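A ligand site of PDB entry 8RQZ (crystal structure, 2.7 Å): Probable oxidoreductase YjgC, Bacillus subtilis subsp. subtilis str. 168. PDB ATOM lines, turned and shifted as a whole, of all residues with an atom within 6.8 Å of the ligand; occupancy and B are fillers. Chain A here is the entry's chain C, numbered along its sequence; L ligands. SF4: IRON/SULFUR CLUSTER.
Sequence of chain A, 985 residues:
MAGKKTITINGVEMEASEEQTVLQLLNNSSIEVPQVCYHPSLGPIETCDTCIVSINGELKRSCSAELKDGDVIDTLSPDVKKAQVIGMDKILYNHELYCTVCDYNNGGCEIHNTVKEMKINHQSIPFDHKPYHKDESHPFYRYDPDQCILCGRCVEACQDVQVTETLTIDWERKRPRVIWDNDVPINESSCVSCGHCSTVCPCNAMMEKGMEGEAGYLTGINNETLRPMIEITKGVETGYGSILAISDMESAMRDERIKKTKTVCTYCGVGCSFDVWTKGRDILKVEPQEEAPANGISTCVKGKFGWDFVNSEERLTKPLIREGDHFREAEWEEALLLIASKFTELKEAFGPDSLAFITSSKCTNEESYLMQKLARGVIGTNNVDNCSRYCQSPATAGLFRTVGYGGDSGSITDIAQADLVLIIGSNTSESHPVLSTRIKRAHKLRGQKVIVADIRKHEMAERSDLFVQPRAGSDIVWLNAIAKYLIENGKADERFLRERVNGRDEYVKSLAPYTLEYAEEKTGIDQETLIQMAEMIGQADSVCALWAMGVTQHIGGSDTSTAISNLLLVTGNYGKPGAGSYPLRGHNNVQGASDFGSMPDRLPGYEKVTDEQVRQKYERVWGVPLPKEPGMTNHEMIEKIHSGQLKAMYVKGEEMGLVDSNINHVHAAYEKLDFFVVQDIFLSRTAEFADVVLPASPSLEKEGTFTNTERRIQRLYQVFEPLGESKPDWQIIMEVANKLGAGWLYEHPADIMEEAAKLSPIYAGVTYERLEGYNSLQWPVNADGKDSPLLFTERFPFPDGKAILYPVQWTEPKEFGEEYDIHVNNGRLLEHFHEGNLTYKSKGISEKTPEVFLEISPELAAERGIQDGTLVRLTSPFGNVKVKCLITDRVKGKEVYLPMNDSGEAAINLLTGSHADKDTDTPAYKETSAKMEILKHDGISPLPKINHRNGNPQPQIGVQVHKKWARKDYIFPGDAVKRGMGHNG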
ATOM      1  N   LEU A  92      13.863  32.402  -5.427  1.00  0.00           N
ATOM      2  CA  LEU A  92      13.934  30.933  -5.391  1.00  0.00           C
ATOM      3  C   LEU A  92      15.299  30.371  -5.767  1.00  0.00           C
ATOM      4  O   LEU A  92      15.649  29.265  -5.348  1.00  0.00           O
ATOM      5  CB  LEU A  92      12.832  30.313  -6.241  1.00  0.00           C
ATOM      6  CG  LEU A  92      11.406  30.523  -5.778  1.00  0.00           C
ATOM      7  CD1 LEU A  92      10.451  29.825  -6.691  1.00  0.00           C
ATOM      8  CD2 LEU A  92      11.212  30.040  -4.358  1.00  0.00           C
ATOM      9  N   HIS A  95      16.936  30.758  -2.446  1.00  0.00           N
ATOM     10  CA  HIS A  95      16.257  30.114  -1.331  1.00  0.00           C
ATOM     11  C   HIS A  95      15.741  28.761  -1.758  1.00  0.00           C
ATOM     12  O   HIS A  95      15.001  28.649  -2.737  1.00  0.00           O
ATOM     13  CB  HIS A  95      15.084  30.973  -0.846  1.00  0.00           C
ATOM     14  CG  HIS A  95      14.335  30.399   0.312  1.00  0.00           C
ATOM     15  ND1 HIS A  95      14.745  30.623   1.605  1.00  0.00           N
ATOM     16  CD2 HIS A  95      13.211  29.649   0.324  1.00  0.00           C
ATOM     17  CE1 HIS A  95      13.874  29.978   2.365  1.00  0.00           C
ATOM     18  NE2 HIS A  95      12.941  29.378   1.647  1.00  0.00           N
ATOM     19  N   GLU A  96      16.084  27.732  -0.986  1.00  0.00           N
ATOM     20  CA  GLU A  96      15.654  26.376  -1.272  1.00  0.00           C
ATOM     21  C   GLU A  96      14.344  26.064  -0.571  1.00  0.00           C
ATOM     22  O   GLU A  96      14.252  26.208   0.650  1.00  0.00           O
ATOM     23  CB  GLU A  96      16.727  25.412  -0.793  1.00  0.00           C
ATOM     24  CG  GLU A  96      16.437  23.954  -1.083  1.00  0.00           C
ATOM     25  CD  GLU A  96      17.640  23.103  -0.778  1.00  0.00           C
ATOM     26  OE1 GLU A  96      18.320  23.383   0.247  1.00  0.00           O
ATOM     27  OE2 GLU A  96      17.924  22.170  -1.554  1.00  0.00           O
ATOM     28  N   LEU A  97      13.336  25.648  -1.335  1.00  0.00           N
ATOM     29  CA  LEU A  97      12.051  25.319  -0.742  1.00  0.00           C
ATOM     30  C   LEU A  97      12.120  23.894  -0.263  1.00  0.00           C
ATOM     31  O   LEU A  97      12.360  22.999  -1.063  1.00  0.00           O
ATOM     32  CB  LEU A  97      10.940  25.456  -1.783  1.00  0.00           C
ATOM     33  CG  LEU A  97      10.690  26.859  -2.306  1.00  0.00           C
ATOM     34  CD1 LEU A  97       9.684  26.840  -3.427  1.00  0.00           C
ATOM     35  CD2 LEU A  97      10.211  27.782  -1.191  1.00  0.00           C
ATOM     36  N   TYR A  98      11.982  23.667   1.037  1.00  0.00           N
ATOM     37  CA  TYR A  98      11.921  22.318   1.613  1.00  0.00           C
ATOM     38  C   TYR A  98      10.897  22.254   2.776  1.00  0.00           C
ATOM     39  O   TYR A  98      11.059  21.465   3.690  1.00  0.00           O
ATOM     40  CB  TYR A  98      13.298  21.773   2.035  1.00  0.00           C
ATOM     41  CG  TYR A  98      14.141  22.689   2.888  1.00  0.00           C
ATOM     42  CD1 TYR A  98      13.967  22.739   4.268  1.00  0.00           C
ATOM     43  CD2 TYR A  98      15.205  23.391   2.344  1.00  0.00           C
ATOM     44  CE1 TYR A  98      14.770  23.555   5.064  1.00  0.00           C
ATOM     45  CE2 TYR A  98      16.022  24.188   3.132  1.00  0.00           C
ATOM     46  CZ  TYR A  98      15.794  24.281   4.496  1.00  0.00           C
ATOM     47  OH  TYR A  98      16.607  25.070   5.273  1.00  0.00           O
ATOM     48  N   CYS A  99       9.844  23.085   2.670  1.00  0.00           N
ATOM     49  CA  CYS A  99       8.779  23.409   3.593  1.00  0.00           C
ATOM     50  C   CYS A  99       8.323  22.288   4.517  1.00  0.00           C
ATOM     51  O   CYS A  99       8.351  22.515   5.723  1.00  0.00           O
ATOM     52  CB  CYS A  99       7.610  24.005   2.814  1.00  0.00           C
ATOM     53  SG  CYS A  99       8.096  25.261   1.594  1.00  0.00           S
ATOM     54  N   THR A 100       7.962  21.094   4.031  1.00  0.00           N
ATOM     55  CA  THR A 100       7.495  20.005   4.913  1.00  0.00           C
ATOM     56  C   THR A 100       8.495  19.648   6.028  1.00  0.00           C
ATOM     57  O   THR A 100       8.119  19.182   7.103  1.00  0.00           O
ATOM     58  CB  THR A 100       7.105  18.739   4.120  1.00  0.00           C
ATOM     59  OG1 THR A 100       6.461  19.111   2.899  1.00  0.00           O
ATOM     60  CG2 THR A 100       6.188  17.818   4.910  1.00  0.00           C
ATOM     61  N   VAL A 101       9.789  19.875   5.767  1.00  0.00           N
ATOM     62  CA  VAL A 101      10.832  19.609   6.757  1.00  0.00           C
ATOM     63  C   VAL A 101      11.551  20.893   7.188  1.00  0.00           C
ATOM     64  O   VAL A 101      12.696  20.835   7.619  1.00  0.00           O
ATOM     65  CB  VAL A 101      11.811  18.513   6.275  1.00  0.00           C
ATOM     66  CG1 VAL A 101      11.082  17.187   6.125  1.00  0.00           C
ATOM     67  CG2 VAL A 101      12.492  18.897   4.964  1.00  0.00           C
ATOM     68  N   CYS A 102      10.861  22.044   7.131  1.00  0.00           N
ATOM     69  CA  CYS A 102      11.407  23.339   7.511  1.00  0.00           C
ATOM     70  C   CYS A 102      10.634  23.867   8.714  1.00  0.00           C
ATOM     71  O   CYS A 102       9.411  23.816   8.735  1.00  0.00           O
ATOM     72  CB  CYS A 102      11.340  24.326   6.339  1.00  0.00           C
ATOM     73  SG  CYS A 102      11.829  26.017   6.768  1.00  0.00           S
ATOM     74  N   ASP A 103      11.356  24.413   9.698  1.00  0.00           N
ATOM     75  CA  ASP A 103      10.727  24.951  10.909  1.00  0.00           C
ATOM     76  C   ASP A 103       9.970  26.235  10.685  1.00  0.00           C
ATOM     77  O   ASP A 103       9.158  26.584  11.538  1.00  0.00           O
ATOM     78  CB  ASP A 103      11.745  25.113  12.033  1.00  0.00           C
ATOM     79  CG  ASP A 103      12.354  23.776  12.379  1.00  0.00           C
ATOM     80  OD1 ASP A 103      11.660  22.981  13.058  1.00  0.00           O
ATOM     81  OD2 ASP A 103      13.521  23.533  11.984  1.00  0.00           O
ATOM     82  N   TYR A 104      10.202  26.947   9.566  1.00  0.00           N
ATOM     83  CA  TYR A 104       9.488  28.181   9.226  1.00  0.00           C
ATOM     84  C   TYR A 104       8.151  27.938   8.464  1.00  0.00           C
ATOM     85  O   TYR A 104       7.440  28.895   8.130  1.00  0.00           O
ATOM     86  CB  TYR A 104      10.387  29.134   8.444  1.00  0.00           C
ATOM     87  CG  TYR A 104      10.063  30.597   8.669  1.00  0.00           C
ATOM     88  CD1 TYR A 104      10.216  31.175   9.926  1.00  0.00           C
ATOM     89  CD2 TYR A 104       9.636  31.407   7.632  1.00  0.00           C
ATOM     90  CE1 TYR A 104       9.928  32.515  10.134  1.00  0.00           C
ATOM     91  CE2 TYR A 104       9.348  32.747   7.840  1.00  0.00           C
ATOM     92  CZ  TYR A 104       9.538  33.306   9.081  1.00  0.00           C
ATOM     93  OH  TYR A 104       9.258  34.641   9.299  1.00  0.00           O
ATOM     94  N   ASN A 105       7.795  26.677   8.209  1.00  0.00           N
ATOM     95  CA  ASN A 105       6.566  26.332   7.519  1.00  0.00           C
ATOM     96  C   ASN A 105       5.425  26.345   8.558  1.00  0.00           C
ATOM     97  O   ASN A 105       4.829  25.312   8.822  1.00  0.00           O
ATOM     98  CB  ASN A 105       6.739  24.967   6.874  1.00  0.00           C
ATOM     99  CG  ASN A 105       5.547  24.420   6.165  1.00  0.00           C
ATOM    100  OD1 ASN A 105       4.894  25.084   5.370  1.00  0.00           O
ATOM    101  ND2 ASN A 105       5.228  23.171   6.459  1.00  0.00           N
ATOM    102  N   ASN A 106       5.147  27.519   9.167  1.00  0.00           N
ATOM    103  CA  ASN A 106       4.109  27.706  10.182  1.00  0.00           C
ATOM    104  C   ASN A 106       2.960  28.590   9.662  1.00  0.00           C
ATOM    105  O   ASN A 106       2.364  29.342  10.437  1.00  0.00           O
ATOM    106  CB  ASN A 106       4.711  28.356  11.414  1.00  0.00           C
ATOM    107  CG  ASN A 106       5.802  27.553  12.029  1.00  0.00           C
ATOM    108  OD1 ASN A 106       5.609  26.391  12.370  1.00  0.00           O
ATOM    109  ND2 ASN A 106       6.952  28.181  12.200  1.00  0.00           N
ATOM    110  N   CYS A 109       5.115  31.975   6.593  1.00  0.00           N
ATOM    111  CA  CYS A 109       6.315  32.174   5.786  1.00  0.00           C
ATOM    112  C   CYS A 109       6.001  32.930   4.510  1.00  0.00           C
ATOM    113  O   CYS A 109       5.283  32.416   3.659  1.00  0.00           O
ATOM    114  CB  CYS A 109       6.995  30.852   5.476  1.00  0.00           C
ATOM    115  SG  CYS A 109       8.531  31.046   4.549  1.00  0.00           S
ATOM    116  N   GLU A 110       6.567  34.132   4.347  1.00  0.00           N
ATOM    117  CA  GLU A 110       6.315  34.981   3.191  1.00  0.00           C
ATOM    118  C   GLU A 110       6.814  34.398   1.872  1.00  0.00           C
ATOM    119  O   GLU A 110       6.152  34.637   0.858  1.00  0.00           O
ATOM    120  CB  GLU A 110       6.833  36.397   3.407  1.00  0.00           C
ATOM    121  CG  GLU A 110       5.879  37.155   4.310  1.00  0.00           C
ATOM    122  CD  GLU A 110       6.474  38.309   5.076  1.00  0.00           C
ATOM    123  OE1 GLU A 110       7.027  38.078   6.178  1.00  0.00           O
ATOM    124  OE2 GLU A 110       6.351  39.454   4.585  1.00  0.00           O
ATOM    125  N   ILE A 111       7.894  33.610   1.851  1.00  0.00           N
ATOM    126  CA  ILE A 111       8.326  32.965   0.614  1.00  0.00           C
ATOM    127  C   ILE A 111       7.315  31.859   0.282  1.00  0.00           C
ATOM    128  O   ILE A 111       6.762  31.826  -0.824  1.00  0.00           O
ATOM    129  CB  ILE A 111       9.771  32.434   0.702  1.00  0.00           C
ATOM    130  CG1 ILE A 111      10.751  33.615   0.770  1.00  0.00           C
ATOM    131  CG2 ILE A 111      10.085  31.472  -0.473  1.00  0.00           C
ATOM    132  CD1 ILE A 111      12.169  33.237   0.847  1.00  0.00           C
ATOM    133  N   HIS A 112       7.012  31.015   1.259  1.00  0.00           N
ATOM    134  CA  HIS A 112       6.063  29.929   1.095  1.00  0.00           C
ATOM    135  C   HIS A 112       4.697  30.394   0.583  1.00  0.00           C
ATOM    136  O   HIS A 112       4.261  29.911  -0.456  1.00  0.00           O
ATOM    137  CB  HIS A 112       5.930  29.146   2.407  1.00  0.00           C
ATOM    138  CG  HIS A 112       4.985  27.981   2.323  1.00  0.00           C
ATOM    139  ND1 HIS A 112       3.669  28.088   2.728  1.00  0.00           N
ATOM    140  CD2 HIS A 112       5.208  26.722   1.867  1.00  0.00           C
ATOM    141  CE1 HIS A 112       3.133  26.902   2.503  1.00  0.00           C
ATOM    142  NE2 HIS A 112       4.011  26.049   1.992  1.00  0.00           N
ATOM    143  N   ASN A 113       4.056  31.352   1.265  1.00  0.00           N
ATOM    144  CA  ASN A 113       2.754  31.844   0.831  1.00  0.00           C
ATOM    145  C   ASN A 113       2.819  32.653  -0.458  1.00  0.00           C
ATOM    146  O   ASN A 113       1.789  32.790  -1.096  1.00  0.00           O
ATOM    147  CB  ASN A 113       2.047  32.658   1.886  1.00  0.00           C
ATOM    148  CG  ASN A 113       2.162  32.231   3.314  1.00  0.00           C
ATOM    149  OD1 ASN A 113       2.351  31.058   3.691  1.00  0.00           O
ATOM    150  ND2 ASN A 113       2.021  33.228   4.159  1.00  0.00           N
ATOM    151  N   VAL A 115       4.938  31.891  -3.082  1.00  0.00           N
ATOM    152  CA  VAL A 115       4.999  30.840  -4.109  1.00  0.00           C
ATOM    153  C   VAL A 115       3.609  30.211  -4.309  1.00  0.00           C
ATOM    154  O   VAL A 115       3.208  29.911  -5.441  1.00  0.00           O
ATOM    155  CB  VAL A 115       6.068  29.784  -3.753  1.00  0.00           C
ATOM    156  CG1 VAL A 115       5.981  28.577  -4.679  1.00  0.00           C
ATOM    157  CG2 VAL A 115       7.456  30.387  -3.775  1.00  0.00           C
ATOM    158  N   GLN A 147      19.801  29.896   2.334  1.00  0.00           N
ATOM    159  CA  GLN A 147      18.372  30.258   2.367  1.00  0.00           C
ATOM    160  C   GLN A 147      18.134  31.782   2.250  1.00  0.00           C
ATOM    161  O   GLN A 147      16.995  32.214   2.118  1.00  0.00           O
ATOM    162  CB  GLN A 147      17.719  29.756   3.659  1.00  0.00           C
ATOM    163  CG  GLN A 147      17.749  28.256   3.800  1.00  0.00           C
ATOM    164  CD  GLN A 147      16.917  27.582   2.741  1.00  0.00           C
ATOM    165  OE1 GLN A 147      17.432  27.017   1.787  1.00  0.00           O
ATOM    166  NE2 GLN A 147      15.611  27.635   2.894  1.00  0.00           N
ATOM    167  N   PRO A 202      11.838  37.167   6.209  1.00  0.00           N
ATOM    168  CA  PRO A 202      10.655  36.501   5.630  1.00  0.00           C
ATOM    169  C   PRO A 202      10.747  34.982   5.436  1.00  0.00           C
ATOM    170  O   PRO A 202       9.792  34.387   4.947  1.00  0.00           O
ATOM    171  CB  PRO A 202      10.487  37.193   4.270  1.00  0.00           C
ATOM    172  CG  PRO A 202      11.877  37.606   3.893  1.00  0.00           C
ATOM    173  CD  PRO A 202      12.589  37.936   5.195  1.00  0.00           C
ATOM    174  N   CYS A 203      11.884  34.362   5.757  1.00  0.00           N
ATOM    175  CA  CYS A 203      12.047  32.915   5.603  1.00  0.00           C
ATOM    176  C   CYS A 203      12.868  32.297   6.782  1.00  0.00           C
ATOM    177  O   CYS A 203      12.890  32.895   7.863  1.00  0.00           O
ATOM    178  CB  CYS A 203      12.625  32.580   4.228  1.00  0.00           C
ATOM    179  SG  CYS A 203      14.244  33.321   3.894  1.00  0.00           S
ATOM    180  N   ASN A 204      13.464  31.102   6.625  1.00  0.00           N
ATOM    181  CA  ASN A 204      14.264  30.505   7.691  1.00  0.00           C
ATOM    182  C   ASN A 204      15.751  30.929   7.628  1.00  0.00           C
ATOM    183  O   ASN A 204      16.539  30.397   8.411  1.00  0.00           O
ATOM    184  CB  ASN A 204      14.136  28.988   7.712  1.00  0.00           C
ATOM    185  CG  ASN A 204      14.819  28.312   6.546  1.00  0.00           C
ATOM    186  OD1 ASN A 204      14.860  28.831   5.440  1.00  0.00           O
ATOM    187  ND2 ASN A 204      15.365  27.124   6.775  1.00  0.00           N
ATOM    188  N   ALA A 205      16.142  31.856   6.713  1.00  0.00           N
ATOM    189  CA  ALA A 205      17.514  32.320   6.536  1.00  0.00           C
ATOM    190  C   ALA A 205      18.071  32.863   7.832  1.00  0.00           C
ATOM    191  O   ALA A 205      19.191  32.548   8.206  1.00  0.00           O
ATOM    192  CB  ALA A 205      17.575  33.366   5.451  1.00  0.00           C
ATOM    193  N   LEU A 244       3.501  21.611  -1.979  1.00  0.00           N
ATOM    194  CA  LEU A 244       3.088  22.738  -1.135  1.00  0.00           C
ATOM    195  C   LEU A 244       1.828  22.345  -0.369  1.00  0.00           C
ATOM    196  O   LEU A 244       1.677  22.772   0.768  1.00  0.00           O
ATOM    197  CB  LEU A 244       2.831  24.009  -1.953  1.00  0.00           C
ATOM    198  CG  LEU A 244       4.014  24.964  -2.065  1.00  0.00           C
ATOM    199  CD1 LEU A 244       3.752  26.039  -3.108  1.00  0.00           C
ATOM    200  CD2 LEU A 244       4.342  25.599  -0.735  1.00  0.00           C
ATOM    201  N   SER A 247       2.978  20.116   2.448  1.00  0.00           N
ATOM    202  CA  SER A 247       3.580  20.968   3.472  1.00  0.00           C
ATOM    203  C   SER A 247       2.538  21.788   4.234  1.00  0.00           C
ATOM    204  O   SER A 247       2.755  22.096   5.404  1.00  0.00           O
ATOM    205  CB  SER A 247       4.609  21.893   2.836  1.00  0.00           C
ATOM    206  OG  SER A 247       4.015  22.934   2.085  1.00  0.00           O
HETATM  207 FE1  SF4 L   1       9.418  29.192   4.125  1.00  0.00          FE
HETATM  208 FE2  SF4 L   1       9.372  26.843   2.702  1.00  0.00          FE
HETATM  209 FE3  SF4 L   1      10.806  27.024   5.046  1.00  0.00          FE
HETATM  210 FE4  SF4 L   1      11.671  28.315   2.795  1.00  0.00          FE
HETATM  211  S1  SF4 L   1      11.502  26.065   3.061  1.00  0.00           S
HETATM  212  S2  SF4 L   1      11.563  29.161   4.941  1.00  0.00           S
HETATM  213  S3  SF4 L   1       9.668  28.934   1.844  1.00  0.00           S
HETATM  214  S4  SF4 L   1       8.520  27.211   4.820  1.00  0.00           S
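An iron atom (FE4) of the ligand is bound by a ring nitrogen (NE2) of His 95, at 2.0 Å. FE1 of the ligand is bound by SG of Cys 109, at 2.1 Å. FE3 of the ligand is bound by SG of Cys 102, 2.2 Å away. The backbone NH (N) of Cys 99 lies close to a sulfur (S1) of the ligand, 3.4 Å away. The side-chain sulfur (SG) of Cys 99 is bound to an iron atom (FE2) of the ligand. A sulfur (S1) of the ligand lies close to the backbone NH (N) of Tyr 98, at 3.2 Å. N of Asn 204 lies close to S2 of the ligand, at 3.2 Å. OD1 of Asn 204 sits close to S2 of the ligand, 3.4 Å away. N of His 112 lies close to S3 of the ligand (3.4 Å). A sulfur (S4) of the ligand lies close to the backbone NH of Asn 105 (3.5 Å).
ND1 of His 95 sits at hydrogen-bond distance from SG of Cys 203 (3.6 Å). N of His 112 sits close to SG of Cys 109 (3.6 Å). The side-chain amide nitrogen of Asn 204 sits close to the side-chain sulfur of Cys 102. The side-chain amide nitrogen of Asn 105 sits close to the backbone carbonyl oxygen of Cys 99 (3.3 Å). The side-chain amide oxygen of Asn 204 sits at hydrogen-bond distance from the side-chain amide nitrogen of Gln 147 (2.9 Å). A ring nitrogen (NE2) of His 112 is in hydrogen-bond range of the side-chain hydroxyl of Ser 247 (3.1 Å). N of Ala 205 lies close to SG of Cys 203 (3.7 Å). The side-chain amide nitrogen (NE2) of Gln 147 lies within hydrogen-bond range of the backbone carbonyl oxygen (O) of Glu 96.
O of Glu 96 lies close to S1 of the ligand (3.7 Å). Merely in contact with the ligand: Leu 97 (3.3 Å), Ile 111 (3.5 Å), Cys 203 (3.7 Å), Tyr 104 (3.7 Å) and Gln 147 (3.999 Å). Hydrophobic or aromatic side chains that line the ligand: His 95, Leu 97, Tyr 104, Ile 111 and His 112.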
